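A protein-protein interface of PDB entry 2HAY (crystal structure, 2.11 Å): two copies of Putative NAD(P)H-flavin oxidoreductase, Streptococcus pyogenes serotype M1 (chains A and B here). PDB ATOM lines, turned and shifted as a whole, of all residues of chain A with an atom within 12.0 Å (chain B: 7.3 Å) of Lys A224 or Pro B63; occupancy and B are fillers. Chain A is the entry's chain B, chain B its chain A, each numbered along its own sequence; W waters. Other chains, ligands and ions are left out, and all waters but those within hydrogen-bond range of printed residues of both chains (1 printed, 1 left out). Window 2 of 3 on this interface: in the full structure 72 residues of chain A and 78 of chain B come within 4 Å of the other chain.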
ATOM      1  N   MET A 220      15.604  36.333  27.142  1.00  0.00           N
ATOM      2  CA  MET A 220      14.929  35.211  26.460  1.00  0.00           C
ATOM      3  C   MET A 220      15.492  33.829  26.836  1.00  0.00           C
ATOM      4  O   MET A 220      16.688  33.680  27.022  1.00  0.00           O
ATOM      5  CB  MET A 220      14.935  35.405  24.928  1.00  0.00           C
ATOM      6  CG  MET A 220      16.302  35.495  24.282  1.00  0.00           C
ATOM      7  SD  MET A 220      16.264  35.407  22.324  1.00  0.00           S
ATOM      8  CE  MET A 220      15.965  37.266  21.872  1.00  0.00           C
ATOM      9  N   SER A 221      14.614  32.831  26.950  1.00  0.00           N
ATOM     10  CA  SER A 221      14.992  31.480  27.330  1.00  0.00           C
ATOM     11  C   SER A 221      13.957  30.459  26.865  1.00  0.00           C
ATOM     12  O   SER A 221      12.861  30.821  26.438  1.00  0.00           O
ATOM     13  CB  SER A 221      15.185  31.359  28.846  1.00  0.00           C
ATOM     14  OG  SER A 221      13.961  31.551  29.529  1.00  0.00           O
ATOM     15  N   VAL A 222      14.332  29.187  26.946  1.00  0.00           N
ATOM     16  CA  VAL A 222      13.477  28.081  26.552  1.00  0.00           C
ATOM     17  C   VAL A 222      13.329  27.150  27.747  1.00  0.00           C
ATOM     18  O   VAL A 222      14.325  26.761  28.355  1.00  0.00           O
ATOM     19  CB  VAL A 222      14.070  27.301  25.329  1.00  0.00           C
ATOM     20  CG1 VAL A 222      13.213  26.118  24.966  1.00  0.00           C
ATOM     21  CG2 VAL A 222      14.212  28.226  24.131  1.00  0.00           C
ATOM     22  N   VAL A 223      12.085  26.823  28.088  1.00  0.00           N
ATOM     23  CA  VAL A 223      11.789  25.765  29.039  1.00  0.00           C
ATOM     24  C   VAL A 223      11.449  24.489  28.250  1.00  0.00           C
ATOM     25  O   VAL A 223      10.377  24.381  27.642  1.00  0.00           O
ATOM     26  CB  VAL A 223      10.677  26.163  30.075  1.00  0.00           C
ATOM     27  CG1 VAL A 223      10.365  24.990  31.032  1.00  0.00           C
ATOM     28  CG2 VAL A 223      11.130  27.331  30.902  1.00  0.00           C
ATOM     29  N   LYS A 224      12.424  23.574  28.248  1.00  0.00           N
ATOM     30  CA  LYS A 224      12.385  22.198  27.696  1.00  0.00           C
ATOM     31  C   LYS A 224      12.960  22.039  26.302  1.00  0.00           C
ATOM     32  O   LYS A 224      13.993  21.398  26.156  1.00  0.00           O
ATOM     33  CB  LYS A 224      11.048  21.435  27.905  1.00  0.00           C
ATOM     34  CG  LYS A 224      10.774  20.265  26.965  1.00  0.00           C
ATOM     35  CD  LYS A 224      10.297  19.007  27.745  1.00  0.00           C
ATOM     36  CE  LYS A 224       9.561  17.968  26.880  1.00  0.00           C
ATOM     37  NZ  LYS A 224       8.068  18.199  26.836  1.00  0.00           N
ATOM     38  N   VAL B  58      10.070  30.754  26.088  1.00  0.00           N
ATOM     39  CA  VAL B  58       9.460  29.784  25.205  1.00  0.00           C
ATOM     40  C   VAL B  58       9.137  28.529  26.023  1.00  0.00           C
ATOM     41  O   VAL B  58      10.037  27.860  26.546  1.00  0.00           O
ATOM     42  CB  VAL B  58      10.412  29.481  24.005  1.00  0.00           C
ATOM     43  CG1 VAL B  58       9.801  28.489  23.037  1.00  0.00           C
ATOM     44  CG2 VAL B  58      10.753  30.769  23.304  1.00  0.00           C
ATOM     45  N   LEU B  59       7.848  28.227  26.166  1.00  0.00           N
ATOM     46  CA  LEU B  59       7.432  27.086  26.958  1.00  0.00           C
ATOM     47  C   LEU B  59       7.181  25.903  26.033  1.00  0.00           C
ATOM     48  O   LEU B  59       6.088  25.743  25.490  1.00  0.00           O
ATOM     49  CB  LEU B  59       6.193  27.406  27.822  1.00  0.00           C
ATOM     50  CG  LEU B  59       5.660  26.331  28.797  1.00  0.00           C
ATOM     51  CD1 LEU B  59       6.685  26.024  29.915  1.00  0.00           C
ATOM     52  CD2 LEU B  59       4.305  26.770  29.415  1.00  0.00           C
ATOM     53  N   ASP B  60       8.211  25.086  25.847  1.00  0.00           N
ATOM     54  CA  ASP B  60       8.075  23.864  25.054  1.00  0.00           C
ATOM     55  C   ASP B  60       7.650  22.668  25.908  1.00  0.00           C
ATOM     56  O   ASP B  60       7.085  21.699  25.392  1.00  0.00           O
ATOM     57  CB  ASP B  60       9.374  23.561  24.286  1.00  0.00           C
ATOM     58  CG  ASP B  60       9.537  24.425  23.026  1.00  0.00           C
ATOM     59  OD1 ASP B  60       8.523  24.903  22.463  1.00  0.00           O
ATOM     60  OD2 ASP B  60      10.693  24.608  22.575  1.00  0.00           O
ATOM     61  N   ASN B  61       7.902  22.750  27.214  1.00  0.00           N
ATOM     62  CA  ASN B  61       7.611  21.667  28.137  1.00  0.00           C
ATOM     63  C   ASN B  61       6.138  21.352  28.180  1.00  0.00           C
ATOM     64  O   ASN B  61       5.338  22.199  28.583  1.00  0.00           O
ATOM     65  CB  ASN B  61       8.124  22.008  29.534  1.00  0.00           C
ATOM     66  CG  ASN B  61       8.042  20.825  30.487  1.00  0.00           C
ATOM     67  OD1 ASN B  61       7.008  20.581  31.107  1.00  0.00           O
ATOM     68  ND2 ASN B  61       9.131  20.088  30.607  1.00  0.00           N
ATOM     69  N   LYS B  62       5.786  20.135  27.760  1.00  0.00           N
ATOM     70  CA  LYS B  62       4.382  19.737  27.610  1.00  0.00           C
ATOM     71  C   LYS B  62       3.668  19.464  28.933  1.00  0.00           C
ATOM     72  O   LYS B  62       2.500  19.845  29.072  1.00  0.00           O
ATOM     73  CB  LYS B  62       4.227  18.571  26.625  1.00  0.00           C
ATOM     74  CG  LYS B  62       4.620  18.942  25.176  1.00  0.00           C
ATOM     75  CD  LYS B  62       4.244  17.846  24.186  1.00  0.00           C
ATOM     76  CE  LYS B  62       4.835  18.096  22.798  1.00  0.00           C
ATOM     77  NZ  LYS B  62       4.205  19.303  22.147  1.00  0.00           N
ATOM     78  N   PRO B  63       4.337  18.792  29.900  1.00  0.00           N
ATOM     79  CA  PRO B  63       3.684  18.680  31.210  1.00  0.00           C
ATOM     80  C   PRO B  63       3.311  20.008  31.883  1.00  0.00           C
ATOM     81  O   PRO B  63       2.244  20.090  32.487  1.00  0.00           O
ATOM     82  CB  PRO B  63       4.702  17.883  32.050  1.00  0.00           C
ATOM     83  CG  PRO B  63       5.431  17.080  31.035  1.00  0.00           C
ATOM     84  CD  PRO B  63       5.605  18.040  29.887  1.00  0.00           C
ATOM     85  N   ILE B  64       4.164  21.029  31.790  1.00  0.00           N
ATOM     86  CA  ILE B  64       3.842  22.332  32.385  1.00  0.00           C
ATOM     87  C   ILE B  64       2.610  22.958  31.704  1.00  0.00           C
ATOM     88  O   ILE B  64       1.720  23.500  32.377  1.00  0.00           O
ATOM     89  CB  ILE B  64       5.043  23.315  32.378  1.00  0.00           C
ATOM     90  CG1 ILE B  64       6.184  22.752  33.245  1.00  0.00           C
ATOM     91  CG2 ILE B  64       4.599  24.702  32.856  1.00  0.00           C
ATOM     92  CD1 ILE B  64       7.516  23.517  33.128  1.00  0.00           C
ATOM     93  N   LYS B  65       2.545  22.836  30.382  1.00  0.00           N
ATOM     94  CA  LYS B  65       1.390  23.277  29.623  1.00  0.00           C
ATOM     95  C   LYS B  65       0.113  22.579  30.099  1.00  0.00           C
ATOM     96  O   LYS B  65      -0.925  23.228  30.279  1.00  0.00           O
ATOM     97  CB  LYS B  65       1.604  23.023  28.144  1.00  0.00           C
ATOM     98  CG  LYS B  65       2.674  23.881  27.536  1.00  0.00           C
ATOM     99  CD  LYS B  65       2.501  23.861  26.035  1.00  0.00           C
ATOM    100  CE  LYS B  65       3.781  23.500  25.344  1.00  0.00           C
ATOM    101  NZ  LYS B  65       3.578  23.633  23.859  1.00  0.00           N
ATOM    102  N   GLU B  66       0.205  21.265  30.309  1.00  0.00           N
ATOM    103  CA  GLU B  66      -0.912  20.485  30.825  1.00  0.00           C
ATOM    104  C   GLU B  66      -1.379  20.953  32.209  1.00  0.00           C
ATOM    105  O   GLU B  66      -2.576  20.955  32.483  1.00  0.00           O
ATOM    106  CB  GLU B  66      -0.565  18.985  30.867  1.00  0.00           C
ATOM    107  CG  GLU B  66      -0.617  18.301  29.519  1.00  0.00           C
ATOM    108  CD  GLU B  66      -2.011  18.321  28.901  1.00  0.00           C
ATOM    109  OE1 GLU B  66      -3.008  18.015  29.610  1.00  0.00           O
ATOM    110  OE2 GLU B  66      -2.101  18.631  27.692  1.00  0.00           O
ATOM    111  N   GLU B  67      -0.439  21.334  33.067  1.00  0.00           N
ATOM    112  CA  GLU B  67      -0.763  21.844  34.393  1.00  0.00           C
ATOM    113  C   GLU B  67      -1.465  23.183  34.354  1.00  0.00           C
ATOM    114  O   GLU B  67      -2.400  23.420  35.114  1.00  0.00           O
ATOM    115  CB  GLU B  67       0.494  21.989  35.226  1.00  0.00           C
ATOM    116  CG  GLU B  67       1.039  20.685  35.710  1.00  0.00           C
ATOM    117  CD  GLU B  67       2.125  20.906  36.702  1.00  0.00           C
ATOM    118  OE1 GLU B  67       3.246  20.398  36.488  1.00  0.00           O
ATOM    119  OE2 GLU B  67       1.855  21.626  37.675  1.00  0.00           O
ATOM    120  N   ILE B  68      -1.009  24.046  33.448  1.00  0.00           N
ATOM    121  CA  ILE B  68      -1.573  25.376  33.268  1.00  0.00           C
ATOM    122  C   ILE B  68      -2.986  25.322  32.680  1.00  0.00           C
ATOM    123  O   ILE B  68      -3.851  26.109  33.054  1.00  0.00           O
ATOM    124  CB  ILE B  68      -0.674  26.221  32.345  1.00  0.00           C
ATOM    125  CG1 ILE B  68       0.605  26.626  33.080  1.00  0.00           C
ATOM    126  CG2 ILE B  68      -1.443  27.439  31.809  1.00  0.00           C
ATOM    127  CD1 ILE B  68       1.670  27.261  32.148  1.00  0.00           C
ATOM    128  N   LYS B  69      -3.205  24.399  31.756  1.00  0.00           N
ATOM    129  CA  LYS B  69      -4.473  24.311  31.035  1.00  0.00           C
ATOM    130  C   LYS B  69      -5.770  24.473  31.848  1.00  0.00           C
ATOM    131  O   LYS B  69      -6.605  25.279  31.468  1.00  0.00           O
ATOM    132  CB  LYS B  69      -4.534  23.027  30.221  1.00  0.00           C
ATOM    133  CG  LYS B  69      -4.516  23.247  28.745  1.00  0.00           C
ATOM    134  CD  LYS B  69      -4.912  21.961  28.086  1.00  0.00           C
ATOM    135  CE  LYS B  69      -3.779  21.390  27.293  1.00  0.00           C
ATOM    136  NZ  LYS B  69      -4.195  20.025  26.906  1.00  0.00           N
ATOM    137  N   ILE B 180       2.360  27.667  39.710  1.00  0.00           N
ATOM    138  CA  ILE B 180       2.812  26.529  38.879  1.00  0.00           C
ATOM    139  C   ILE B 180       4.181  26.861  38.286  1.00  0.00           C
ATOM    140  O   ILE B 180       5.085  26.036  38.288  1.00  0.00           O
ATOM    141  CB  ILE B 180       1.849  26.267  37.690  1.00  0.00           C
ATOM    142  CG1 ILE B 180       0.406  26.016  38.165  1.00  0.00           C
ATOM    143  CG2 ILE B 180       2.396  25.171  36.741  1.00  0.00           C
ATOM    144  CD1 ILE B 180       0.000  24.634  38.167  1.00  0.00           C
ATOM    145  N   HIS B 184       8.002  25.029  39.263  1.00  0.00           N
ATOM    146  CA  HIS B 184       8.889  24.455  38.272  1.00  0.00           C
ATOM    147  C   HIS B 184      10.155  25.289  38.074  1.00  0.00           C
ATOM    148  O   HIS B 184      10.938  25.011  37.175  1.00  0.00           O
ATOM    149  CB  HIS B 184       8.143  24.279  36.960  1.00  0.00           C
ATOM    150  CG  HIS B 184       7.231  23.101  36.959  1.00  0.00           C
ATOM    151  ND1 HIS B 184       7.681  21.812  36.764  1.00  0.00           N
ATOM    152  CD2 HIS B 184       5.896  23.013  37.143  1.00  0.00           C
ATOM    153  CE1 HIS B 184       6.657  20.980  36.819  1.00  0.00           C
ATOM    154  NE2 HIS B 184       5.563  21.684  37.052  1.00  0.00           N
HETATM  155  O   HOH W   1      12.743  22.884  23.447  1.00  0.00           O
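Val B58 touches Val A222.
Asp B60 touches Val A222.
C of Leu B59 touches O of Val A223 (3.9 Å).
CG1 of Val A223 touches CD1 of Ile B64 (3.8 Å).
O of Asp B60 touches NZ of Lys A224, 3.9 Å away.
Lys A224 touches Asn B61.
Lys A224 touches Pro B63.
Printed residues of chain A that touch a printed residue of chain B: Ser A221, Val A222, Val A223 and Lys A224.
Hydrophobic or aromatic side chains of chain A within 4 Å of the printed part of chain B: Val A222 and Val A223.
Hydrophobic or aromatic side chains of chain B within 4 Å of the printed part of chain A: Val B58, Leu B59, Pro B63 and Ile B64.
Among the printed residues, no Asp or Glu carboxylate lies within 4 Å of a Lys or Arg side-chain nitrogen of the other chain.
Of the printed residues of chain B, Ser A221 touches Val B58.
Of the printed residues of chain B, Val A222 touches Val B58 (3.4 Å) and Asp B60 (3.8 Å).
Of the printed residues of chain B, Val A223 touches Val B58, Leu B59, Asp B60, Asn B61 and Ile B64.
Of chain B, only Asp B60, Asn B61, Lys B62 and Pro B63 come within 4 Å of Lys A224.
Of chain A, only Val A223 comes within 4 Å of Leu B59.
Of the printed residues of chain A, Asp B60 touches Val A222 (3.8 Å), Val A223 (2.9 Å) and Lys A224 (3.9 Å).
Lys B62 touches one residue of chain A.
Of chain A, only Lys A224 (3.9 Å) comes within 4 Å of Pro B63.
Lys B65 touches none of the printed residues of chain A.
No residue of chain A comes within 4 Å of Glu B66.
No residue of chain A comes within 4 Å of Glu B67.
Ile B180 touches none of the printed residues of chain A.
The nearest residue of chain B that does not touch Lys A224 is Val B58 (5.2 Å).
No position is printed for both chains.
OD1 of Asn B61 lies within hydrogen-bond range of N of Ile B64 (3.0 Å).
Water W1 lies within hydrogen-bond range of the side-chain carboxylate of Asp B60 (2.8 Å) and the backbone carbonyl oxygen of Lys A224 (3.3 Å).
O of Val B58 sits at hydrogen-bond distance from N of Val A223 (2.8 Å).
N of Asp B60 sits at hydrogen-bond distance from O of Val A223 (2.9 Å).
The side-chain amino group (NZ) of Lys A224 sits close to the backbone NH (N) of Lys B62, 3.1 Å away.
The backbone carbonyl oxygen (O) of Val A223 is in hydrogen-bond range of the backbone NH (N) of Asn B61 (3.0 Å).
The backbone NH (N) of Val B58 lies within hydrogen-bond range of the backbone carbonyl oxygen (O) of Ser A221.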
